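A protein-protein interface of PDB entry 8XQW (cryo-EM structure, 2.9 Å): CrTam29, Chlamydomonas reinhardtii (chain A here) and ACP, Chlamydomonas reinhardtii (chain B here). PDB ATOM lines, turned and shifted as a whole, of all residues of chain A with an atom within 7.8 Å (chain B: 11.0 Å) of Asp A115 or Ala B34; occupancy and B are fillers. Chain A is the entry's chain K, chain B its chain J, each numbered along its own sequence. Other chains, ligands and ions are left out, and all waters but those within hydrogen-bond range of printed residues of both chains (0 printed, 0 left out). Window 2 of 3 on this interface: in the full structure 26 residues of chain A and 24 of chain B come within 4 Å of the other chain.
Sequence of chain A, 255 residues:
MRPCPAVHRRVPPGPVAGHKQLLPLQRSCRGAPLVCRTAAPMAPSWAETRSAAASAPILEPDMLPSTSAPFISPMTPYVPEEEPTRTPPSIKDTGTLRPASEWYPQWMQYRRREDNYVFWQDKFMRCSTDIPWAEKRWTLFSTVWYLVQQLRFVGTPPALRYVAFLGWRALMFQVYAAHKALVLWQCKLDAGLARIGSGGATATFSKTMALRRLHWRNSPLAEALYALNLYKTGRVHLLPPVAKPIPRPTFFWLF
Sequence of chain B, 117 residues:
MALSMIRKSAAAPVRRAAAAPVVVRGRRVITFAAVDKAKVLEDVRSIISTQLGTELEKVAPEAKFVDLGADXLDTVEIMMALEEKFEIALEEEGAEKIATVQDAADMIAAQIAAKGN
Of the printed residues of chain B, Asp A115 touches Ala B33 (2.8 Å) and Ala B34 (3.3 Å). Of chain A, only Arg A111 (3.8 Å), Arg A112 (3.7 Å) and Asp A115 (3.3 Å) come within 4 Å of Ala B34. Of chain B, only Ala B33 (3.9 Å), Ala B34 (3.8 Å), Ile B112 (2.8 Å), Ala B113 (3.5 Å) and Lys B115 (3.7 Å) come within 4 Å of Arg A111. Arg A112 touches one residue of chain B. No residue of chain B comes within 4 Å of Glu A114. No residue of chain B comes within 4 Å of Asn A116. Tyr A117 touches none of the printed residues of chain B. Of chain A, only Arg A111 and Asp A115 come within 4 Å of Ala B33. Printed residues of chain A within 4 Å of Ala B113: Arg A111 (3.5 Å). Printed residues of chain A within 4 Å of Ile B112: Trp A107 and Arg A111. Of the printed residues of chain B, Val A118 touches Gly B116 (3.7 Å). Printed residues of chain A within 4 Å of Lys B39: Tyr A110 (3.6 Å). Printed residues of chain A within 4 Å of Gly B116: Val A118. Arg A113 touches none of the printed residues of chain B. Phe A119 touches none of the printed residues of chain B. The nearest residue of chain B that does not touch Asp A115 is Val B35 (6.2 Å).
Trp A107 touches Ile B112 (CB to CG2, 3.9 Å). Trp A107 touches Lys B115 (CZ3 to CG, 3.8 Å). Val B35 touches Tyr A110. Tyr A110 touches Asp B36. CB of Lys B39 touches CD1 of Tyr A110 (3.6 Å). Arg A111 touches Ala B33 (NH1 to N, 3.9 Å). O of Ala B34 touches CA of Arg A111, at 3.8 Å. Arg A111 touches Lys B115 (NH1 to CB, 3.7 Å). N of Arg A112 touches O of Ala B34 (3.7 Å). CG1 of Val A118 touches CA of Gly B116 (3.7 Å).
Of the 12 printed residues of chain A, 6 touch a printed residue of chain B. Of the 18 printed residues of chain B, 9 touch a printed residue of chain A. Printed residues of chain B that touch a printed residue of chain A: Ala B33, Ala B34, Val B35, Asp B36, Lys B39, Ile B112, Ala B113, Lys B115 and Gly B116. Among the printed residues, 14 pairs touch across the chains.
The backbone carbonyl oxygen (O) of Ile B112 is in hydrogen-bond range of the guanidinium group (NH1) of Arg A111. The backbone carbonyl oxygen of Ala B113 sits at hydrogen-bond distance from the guanidinium group of Arg A111 (3.5 Å). The backbone NH of Ala B34 lies within hydrogen-bond range of the side-chain carboxylate of Asp A115 (3.3 Å). N of Ala B33 is in hydrogen-bond range of OD2 of Asp A115 (2.8 Å).
NZ of Lys B37 is in hydrogen-bond range of O of Val B35, 3.5 Å away. O of Asp A115 lies within hydrogen-bond range of NH2 of Arg A111, at 2.8 Å. The guanidinium group (NE) of Arg A111 sits at hydrogen-bond distance from the side-chain amide oxygen (OD1) of Asn A116, at 3.2 Å. OD2 of Asp A115 lies within salt-bridge range of NE of Arg A112 (3.96 Å).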
ATOM      1  N   TRP A 107     -22.725   5.285  18.664  1.00  0.00           N
ATOM      2  CA  TRP A 107     -21.493   5.853  19.184  1.00  0.00           C
ATOM      3  C   TRP A 107     -21.097   5.242  20.517  1.00  0.00           C
ATOM      4  O   TRP A 107     -19.923   5.290  20.880  1.00  0.00           O
ATOM      5  CB  TRP A 107     -21.633   7.364  19.324  1.00  0.00           C
ATOM      6  CG  TRP A 107     -22.934   7.781  19.870  1.00  0.00           C
ATOM      7  CD1 TRP A 107     -24.065   8.013  19.176  1.00  0.00           C
ATOM      8  CD2 TRP A 107     -23.247   8.010  21.240  1.00  0.00           C
ATOM      9  NE1 TRP A 107     -25.072   8.373  20.023  1.00  0.00           N
ATOM     10  CE2 TRP A 107     -24.591   8.370  21.303  1.00  0.00           C
ATOM     11  CE3 TRP A 107     -22.520   7.929  22.423  1.00  0.00           C
ATOM     12  CZ2 TRP A 107     -25.222   8.660  22.493  1.00  0.00           C
ATOM     13  CZ3 TRP A 107     -23.147   8.215  23.599  1.00  0.00           C
ATOM     14  CH2 TRP A 107     -24.481   8.577  23.630  1.00  0.00           C
ATOM     15  N   MET A 108     -22.043   4.642  21.231  1.00  0.00           N
ATOM     16  CA  MET A 108     -21.745   4.064  22.533  1.00  0.00           C
ATOM     17  C   MET A 108     -20.638   3.030  22.462  1.00  0.00           C
ATOM     18  O   MET A 108     -20.000   2.740  23.474  1.00  0.00           O
ATOM     19  CB  MET A 108     -22.996   3.425  23.115  1.00  0.00           C
ATOM     20  CG  MET A 108     -23.667   4.222  24.179  1.00  0.00           C
ATOM     21  SD  MET A 108     -25.106   3.357  24.776  1.00  0.00           S
ATOM     22  CE  MET A 108     -24.522   2.774  26.343  1.00  0.00           C
ATOM     23  N   TYR A 110     -17.791   3.231  20.923  1.00  0.00           N
ATOM     24  CA  TYR A 110     -16.452   3.781  20.783  1.00  0.00           C
ATOM     25  C   TYR A 110     -16.063   4.644  21.966  1.00  0.00           C
ATOM     26  O   TYR A 110     -15.446   5.689  21.783  1.00  0.00           O
ATOM     27  CB  TYR A 110     -16.342   4.581  19.492  1.00  0.00           C
ATOM     28  CG  TYR A 110     -16.834   3.846  18.281  1.00  0.00           C
ATOM     29  CD1 TYR A 110     -16.001   3.023  17.570  1.00  0.00           C
ATOM     30  CD2 TYR A 110     -18.125   3.993  17.841  1.00  0.00           C
ATOM     31  CE1 TYR A 110     -16.440   2.358  16.468  1.00  0.00           C
ATOM     32  CE2 TYR A 110     -18.571   3.331  16.741  1.00  0.00           C
ATOM     33  CZ  TYR A 110     -17.726   2.514  16.059  1.00  0.00           C
ATOM     34  OH  TYR A 110     -18.176   1.847  14.952  1.00  0.00           O
ATOM     35  N   ARG A 111     -16.420   4.237  23.174  1.00  0.00           N
ATOM     36  CA  ARG A 111     -16.180   5.019  24.371  1.00  0.00           C
ATOM     37  C   ARG A 111     -15.899   4.087  25.537  1.00  0.00           C
ATOM     38  O   ARG A 111     -16.175   2.891  25.484  1.00  0.00           O
ATOM     39  CB  ARG A 111     -17.369   5.914  24.700  1.00  0.00           C
ATOM     40  CG  ARG A 111     -17.489   7.120  23.821  1.00  0.00           C
ATOM     41  CD  ARG A 111     -18.865   7.702  23.883  1.00  0.00           C
ATOM     42  NE  ARG A 111     -19.250   8.078  25.232  1.00  0.00           N
ATOM     43  CZ  ARG A 111     -19.224   9.320  25.691  1.00  0.00           C
ATOM     44  NH1 ARG A 111     -18.825  10.298  24.908  1.00  0.00           N
ATOM     45  NH2 ARG A 111     -19.597   9.584  26.927  1.00  0.00           N
ATOM     46  N   ARG A 112     -15.345   4.648  26.599  1.00  0.00           N
ATOM     47  CA  ARG A 112     -15.014   3.850  27.764  1.00  0.00           C
ATOM     48  C   ARG A 112     -16.275   3.436  28.496  1.00  0.00           C
ATOM     49  O   ARG A 112     -17.195   4.231  28.660  1.00  0.00           O
ATOM     50  CB  ARG A 112     -14.120   4.648  28.700  1.00  0.00           C
ATOM     51  CG  ARG A 112     -12.713   4.833  28.223  1.00  0.00           C
ATOM     52  CD  ARG A 112     -11.859   5.264  29.381  1.00  0.00           C
ATOM     53  NE  ARG A 112     -12.553   6.247  30.203  1.00  0.00           N
ATOM     54  CZ  ARG A 112     -12.451   6.321  31.525  1.00  0.00           C
ATOM     55  NH1 ARG A 112     -11.686   5.465  32.182  1.00  0.00           N
ATOM     56  NH2 ARG A 112     -13.119   7.250  32.190  1.00  0.00           N
ATOM     57  N   ARG A 113     -16.305   2.192  28.971  1.00  0.00           N
ATOM     58  CA  ARG A 113     -17.458   1.715  29.724  1.00  0.00           C
ATOM     59  C   ARG A 113     -17.794   2.644  30.876  1.00  0.00           C
ATOM     60  O   ARG A 113     -18.957   2.760  31.271  1.00  0.00           O
ATOM     61  CB  ARG A 113     -17.193   0.313  30.258  1.00  0.00           C
ATOM     62  CG  ARG A 113     -17.320  -0.771  29.237  1.00  0.00           C
ATOM     63  CD  ARG A 113     -16.851  -2.097  29.776  1.00  0.00           C
ATOM     64  NE  ARG A 113     -17.051  -3.161  28.804  1.00  0.00           N
ATOM     65  CZ  ARG A 113     -16.187  -3.455  27.847  1.00  0.00           C
ATOM     66  NH1 ARG A 113     -16.442  -4.431  26.997  1.00  0.00           N
ATOM     67  NH2 ARG A 113     -15.064  -2.773  27.738  1.00  0.00           N
ATOM     68  N   GLU A 114     -16.804   3.297  31.432  1.00  0.00           N
ATOM     69  CA  GLU A 114     -17.072   4.205  32.536  1.00  0.00           C
ATOM     70  C   GLU A 114     -17.363   5.582  32.080  1.00  0.00           C
ATOM     71  O   GLU A 114     -17.354   6.502  32.884  1.00  0.00           O
ATOM     72  CB  GLU A 114     -15.894   4.208  33.509  1.00  0.00           C
ATOM     73  CG  GLU A 114     -14.561   3.876  32.867  1.00  0.00           C
ATOM     74  CD  GLU A 114     -14.219   2.399  32.924  1.00  0.00           C
ATOM     75  OE1 GLU A 114     -13.785   1.843  31.895  1.00  0.00           O
ATOM     76  OE2 GLU A 114     -14.386   1.791  33.996  1.00  0.00           O
ATOM     77  N   ASP A 115     -17.619   5.733  30.784  1.00  0.00           N
ATOM     78  CA  ASP A 115     -18.048   6.991  30.200  1.00  0.00           C
ATOM     79  C   ASP A 115     -19.437   6.934  29.604  1.00  0.00           C
ATOM     80  O   ASP A 115     -19.969   7.981  29.242  1.00  0.00           O
ATOM     81  CB  ASP A 115     -17.081   7.428  29.099  1.00  0.00           C
ATOM     82  CG  ASP A 115     -16.149   8.509  29.551  1.00  0.00           C
ATOM     83  OD1 ASP A 115     -16.357   9.041  30.657  1.00  0.00           O
ATOM     84  OD2 ASP A 115     -15.204   8.827  28.803  1.00  0.00           O
ATOM     85  N   ASN A 116     -20.018   5.750  29.460  1.00  0.00           N
ATOM     86  CA  ASN A 116     -21.332   5.560  28.863  1.00  0.00           C
ATOM     87  C   ASN A 116     -22.432   5.653  29.884  1.00  0.00           C
ATOM     88  O   ASN A 116     -23.528   5.152  29.663  1.00  0.00           O
ATOM     89  CB  ASN A 116     -21.383   4.219  28.155  1.00  0.00           C
ATOM     90  CG  ASN A 116     -20.587   4.208  26.907  1.00  0.00           C
ATOM     91  OD1 ASN A 116     -20.269   5.252  26.365  1.00  0.00           O
ATOM     92  ND2 ASN A 116     -20.253   3.028  26.432  1.00  0.00           N
ATOM     93  N   TYR A 117     -22.176   6.261  31.023  1.00  0.00           N
ATOM     94  CA  TYR A 117     -23.231   6.460  31.995  1.00  0.00           C
ATOM     95  C   TYR A 117     -24.181   7.569  31.590  1.00  0.00           C
ATOM     96  O   TYR A 117     -25.173   7.786  32.284  1.00  0.00           O
ATOM     97  CB  TYR A 117     -22.636   6.777  33.366  1.00  0.00           C
ATOM     98  CG  TYR A 117     -22.056   8.160  33.452  1.00  0.00           C
ATOM     99  CD1 TYR A 117     -20.770   8.415  33.038  1.00  0.00           C
ATOM    100  CD2 TYR A 117     -22.799   9.207  33.939  1.00  0.00           C
ATOM    101  CE1 TYR A 117     -20.247   9.668  33.100  1.00  0.00           C
ATOM    102  CE2 TYR A 117     -22.280  10.460  34.004  1.00  0.00           C
ATOM    103  CZ  TYR A 117     -21.005  10.685  33.584  1.00  0.00           C
ATOM    104  OH  TYR A 117     -20.490  11.949  33.656  1.00  0.00           O
ATOM    105  N   VAL A 118     -23.904   8.276  30.493  1.00  0.00           N
ATOM    106  CA  VAL A 118     -24.718   9.418  30.114  1.00  0.00           C
ATOM    107  C   VAL A 118     -26.025   8.992  29.478  1.00  0.00           C
ATOM    108  O   VAL A 118     -26.969   9.781  29.427  1.00  0.00           O
ATOM    109  CB  VAL A 118     -23.929  10.328  29.174  1.00  0.00           C
ATOM    110  CG1 VAL A 118     -22.764  10.897  29.898  1.00  0.00           C
ATOM    111  CG2 VAL A 118     -23.464   9.555  27.986  1.00  0.00           C
ATOM    112  N   PHE A 119     -26.107   7.753  29.006  1.00  0.00           N
ATOM    113  CA  PHE A 119     -27.362   7.187  28.536  1.00  0.00           C
ATOM    114  C   PHE A 119     -28.441   7.268  29.612  1.00  0.00           C
ATOM    115  O   PHE A 119     -29.447   7.979  29.471  1.00  0.00           O
ATOM    116  CB  PHE A 119     -27.091   5.739  28.139  1.00  0.00           C
ATOM    117  CG  PHE A 119     -28.126   5.124  27.270  1.00  0.00           C
ATOM    118  CD1 PHE A 119     -28.435   5.663  26.051  1.00  0.00           C
ATOM    119  CD2 PHE A 119     -28.749   3.966  27.654  1.00  0.00           C
ATOM    120  CE1 PHE A 119     -29.369   5.075  25.262  1.00  0.00           C
ATOM    121  CE2 PHE A 119     -29.672   3.379  26.866  1.00  0.00           C
ATOM    122  CZ  PHE A 119     -29.987   3.933  25.674  1.00  0.00           C
ATOM    123  N   ALA B  33     -15.553  10.851  26.896  1.00  0.00           N
ATOM    124  CA  ALA B  33     -14.485  11.836  26.916  1.00  0.00           C
ATOM    125  C   ALA B  33     -13.190  11.215  26.418  1.00  0.00           C
ATOM    126  O   ALA B  33     -12.239  11.917  26.085  1.00  0.00           O
ATOM    127  CB  ALA B  33     -14.308  12.395  28.306  1.00  0.00           C
ATOM    128  N   ALA B  34     -13.162   9.890  26.377  1.00  0.00           N
ATOM    129  CA  ALA B  34     -12.013   9.152  25.873  1.00  0.00           C
ATOM    130  C   ALA B  34     -12.481   8.217  24.768  1.00  0.00           C
ATOM    131  O   ALA B  34     -13.272   7.307  25.016  1.00  0.00           O
ATOM    132  CB  ALA B  34     -11.336   8.375  26.999  1.00  0.00           C
ATOM    133  N   VAL B  35     -11.988   8.434  23.561  1.00  0.00           N
ATOM    134  CA  VAL B  35     -12.464   7.717  22.391  1.00  0.00           C
ATOM    135  C   VAL B  35     -11.344   6.848  21.838  1.00  0.00           C
ATOM    136  O   VAL B  35     -10.185   7.259  21.740  1.00  0.00           O
ATOM    137  CB  VAL B  35     -12.987   8.689  21.320  1.00  0.00           C
ATOM    138  CG1 VAL B  35     -13.513   7.934  20.133  1.00  0.00           C
ATOM    139  CG2 VAL B  35     -14.060   9.555  21.903  1.00  0.00           C
ATOM    140  N   ASP B  36     -11.705   5.625  21.467  1.00  0.00           N
ATOM    141  CA  ASP B  36     -10.777   4.702  20.825  1.00  0.00           C
ATOM    142  C   ASP B  36     -10.623   5.151  19.383  1.00  0.00           C
ATOM    143  O   ASP B  36     -11.354   4.717  18.497  1.00  0.00           O
ATOM    144  CB  ASP B  36     -11.293   3.276  20.913  1.00  0.00           C
ATOM    145  CG  ASP B  36     -11.724   2.907  22.308  1.00  0.00           C
ATOM    146  OD1 ASP B  36     -11.743   3.805  23.173  1.00  0.00           O
ATOM    147  OD2 ASP B  36     -12.055   1.727  22.542  1.00  0.00           O
ATOM    148  N   LYS B  37      -9.654   6.031  19.146  1.00  0.00           N
ATOM    149  CA  LYS B  37      -9.472   6.589  17.812  1.00  0.00           C
ATOM    150  C   LYS B  37      -9.142   5.518  16.784  1.00  0.00           C
ATOM    151  O   LYS B  37      -9.422   5.698  15.594  1.00  0.00           O
ATOM    152  CB  LYS B  37      -8.380   7.648  17.853  1.00  0.00           C
ATOM    153  CG  LYS B  37      -8.608   8.657  18.945  1.00  0.00           C
ATOM    154  CD  LYS B  37      -7.341   9.385  19.296  1.00  0.00           C
ATOM    155  CE  LYS B  37      -7.633  10.525  20.243  1.00  0.00           C
ATOM    156  NZ  LYS B  37      -8.993  10.396  20.820  1.00  0.00           N
ATOM    157  N   ALA B  38      -8.572   4.397  17.220  1.00  0.00           N
ATOM    158  CA  ALA B  38      -8.275   3.317  16.291  1.00  0.00           C
ATOM    159  C   ALA B  38      -9.545   2.735  15.684  1.00  0.00           C
ATOM    160  O   ALA B  38      -9.636   2.574  14.461  1.00  0.00           O
ATOM    161  CB  ALA B  38      -7.477   2.229  17.002  1.00  0.00           C
ATOM    162  N   LYS B  39     -10.526   2.401  16.526  1.00  0.00           N
ATOM    163  CA  LYS B  39     -11.787   1.864  16.026  1.00  0.00           C
ATOM    164  C   LYS B  39     -12.460   2.843  15.080  1.00  0.00           C
ATOM    165  O   LYS B  39     -12.965   2.458  14.016  1.00  0.00           O
ATOM    166  CB  LYS B  39     -12.719   1.548  17.192  1.00  0.00           C
ATOM    167  CG  LYS B  39     -12.306   0.389  18.047  1.00  0.00           C
ATOM    168  CD  LYS B  39     -13.479  -0.103  18.866  1.00  0.00           C
ATOM    169  CE  LYS B  39     -14.647  -0.463  17.976  1.00  0.00           C
ATOM    170  NZ  LYS B  39     -15.766  -1.079  18.734  1.00  0.00           N
ATOM    171  N   VAL B  40     -12.498   4.117  15.469  1.00  0.00           N
ATOM    172  CA  VAL B  40     -13.120   5.131  14.630  1.00  0.00           C
ATOM    173  C   VAL B  40     -12.430   5.190  13.281  1.00  0.00           C
ATOM    174  O   VAL B  40     -13.082   5.327  12.243  1.00  0.00           O
ATOM    175  CB  VAL B  40     -13.091   6.495  15.340  1.00  0.00           C
ATOM    176  CG1 VAL B  40     -13.665   7.552  14.450  1.00  0.00           C
ATOM    177  CG2 VAL B  40     -13.854   6.427  16.635  1.00  0.00           C
ATOM    178  N   ILE B 108     -15.020  13.147  13.675  1.00  0.00           N
ATOM    179  CA  ILE B 108     -15.958  12.203  14.262  1.00  0.00           C
ATOM    180  C   ILE B 108     -15.588  11.901  15.704  1.00  0.00           C
ATOM    181  O   ILE B 108     -16.461  11.791  16.570  1.00  0.00           O
ATOM    182  CB  ILE B 108     -16.025  10.930  13.413  1.00  0.00           C
ATOM    183  CG1 ILE B 108     -16.865  11.191  12.175  1.00  0.00           C
ATOM    184  CG2 ILE B 108     -16.626   9.813  14.198  1.00  0.00           C
ATOM    185  CD1 ILE B 108     -17.174   9.960  11.399  1.00  0.00           C
ATOM    186  N   ALA B 109     -14.298  11.765  15.994  1.00  0.00           N
ATOM    187  CA  ALA B 109     -13.910  11.436  17.359  1.00  0.00           C
ATOM    188  C   ALA B 109     -14.168  12.594  18.306  1.00  0.00           C
ATOM    189  O   ALA B 109     -14.590  12.377  19.445  1.00  0.00           O
ATOM    190  CB  ALA B 109     -12.445  11.024  17.403  1.00  0.00           C
ATOM    191  N   ALA B 110     -13.936  13.829  17.859  1.00  0.00           N
ATOM    192  CA  ALA B 110     -14.216  14.970  18.719  1.00  0.00           C
ATOM    193  C   ALA B 110     -15.710  15.156  18.917  1.00  0.00           C
ATOM    194  O   ALA B 110     -16.138  15.749  19.908  1.00  0.00           O
ATOM    195  CB  ALA B 110     -13.597  16.232  18.137  1.00  0.00           C
ATOM    196  N   GLN B 111     -16.520  14.673  17.974  1.00  0.00           N
ATOM    197  CA  GLN B 111     -17.967  14.711  18.169  1.00  0.00           C
ATOM    198  C   GLN B 111     -18.414  13.655  19.168  1.00  0.00           C
ATOM    199  O   GLN B 111     -19.174  13.953  20.090  1.00  0.00           O
ATOM    200  CB  GLN B 111     -18.688  14.511  16.841  1.00  0.00           C
ATOM    201  CG  GLN B 111     -18.632  15.701  15.937  1.00  0.00           C
ATOM    202  CD  GLN B 111     -19.103  16.939  16.626  1.00  0.00           C
ATOM    203  OE1 GLN B 111     -20.198  16.974  17.175  1.00  0.00           O
ATOM    204  NE2 GLN B 111     -18.275  17.970  16.615  1.00  0.00           N
ATOM    205  N   ILE B 112     -17.948  12.419  19.000  1.00  0.00           N
ATOM    206  CA  ILE B 112     -18.337  11.348  19.909  1.00  0.00           C
ATOM    207  C   ILE B 112     -17.879  11.655  21.324  1.00  0.00           C
ATOM    208  O   ILE B 112     -18.558  11.317  22.295  1.00  0.00           O
ATOM    209  CB  ILE B 112     -17.784   9.995  19.430  1.00  0.00           C
ATOM    210  CG1 ILE B 112     -18.280   9.662  18.036  1.00  0.00           C
ATOM    211  CG2 ILE B 112     -18.209   8.900  20.355  1.00  0.00           C
ATOM    212  CD1 ILE B 112     -17.839   8.312  17.579  1.00  0.00           C
ATOM    213  N   ALA B 113     -16.723  12.298  21.469  1.00  0.00           N
ATOM    214  CA  ALA B 113     -16.202  12.559  22.805  1.00  0.00           C
ATOM    215  C   ALA B 113     -17.083  13.536  23.563  1.00  0.00           C
ATOM    216  O   ALA B 113     -17.284  13.389  24.771  1.00  0.00           O
ATOM    217  CB  ALA B 113     -14.777  13.091  22.719  1.00  0.00           C
ATOM    218  N   ALA B 114     -17.616  14.537  22.878  1.00  0.00           N
ATOM    219  CA  ALA B 114     -18.429  15.569  23.517  1.00  0.00           C
ATOM    220  C   ALA B 114     -19.912  15.250  23.378  1.00  0.00           C
ATOM    221  O   ALA B 114     -20.666  15.962  22.731  1.00  0.00           O
ATOM    222  CB  ALA B 114     -18.105  16.932  22.924  1.00  0.00           C
ATOM    223  N   LYS B 115     -20.331  14.164  24.017  1.00  0.00           N
ATOM    224  CA  LYS B 115     -21.694  13.671  23.886  1.00  0.00           C
ATOM    225  C   LYS B 115     -22.515  13.847  25.147  1.00  0.00           C
ATOM    226  O   LYS B 115     -23.658  14.295  25.081  1.00  0.00           O
ATOM    227  CB  LYS B 115     -21.686  12.200  23.488  1.00  0.00           C
ATOM    228  CG  LYS B 115     -22.771  11.844  22.522  1.00  0.00           C
ATOM    229  CD  LYS B 115     -22.627  12.649  21.272  1.00  0.00           C
ATOM    230  CE  LYS B 115     -23.731  12.355  20.296  1.00  0.00           C
ATOM    231  NZ  LYS B 115     -25.052  12.712  20.848  1.00  0.00           N
ATOM    232  N   GLY B 116     -21.974  13.488  26.303  1.00  0.00           N
ATOM    233  CA  GLY B 116     -22.720  13.691  27.531  1.00  0.00           C
ATOM    234  C   GLY B 116     -22.989  15.155  27.809  1.00  0.00           C
ATOM    235  O   GLY B 116     -24.141  15.582  27.870  1.00  0.00           O
ATOM    236  N   ASN B 117     -21.931  15.941  27.954  1.00  0.00           N
ATOM    237  CA  ASN B 117     -22.046  17.372  28.197  1.00  0.00           C
ATOM    238  C   ASN B 117     -22.483  18.135  26.950  1.00  0.00           C
ATOM    239  O   ASN B 117     -21.892  18.004  25.880  1.00  0.00           O
ATOM    240  CB  ASN B 117     -20.714  17.923  28.693  1.00  0.00           C
ATOM    241  CG  ASN B 117     -19.562  17.550  27.789  1.00  0.00           C
ATOM    242  OD1 ASN B 117     -19.276  18.241  26.814  1.00  0.00           O
ATOM    243  ND2 ASN B 117     -18.895  16.445  28.107  1.00  0.00           N
ATOM    244  OXT ASN B 117     -23.433  18.914  26.986  1.00  0.00           O
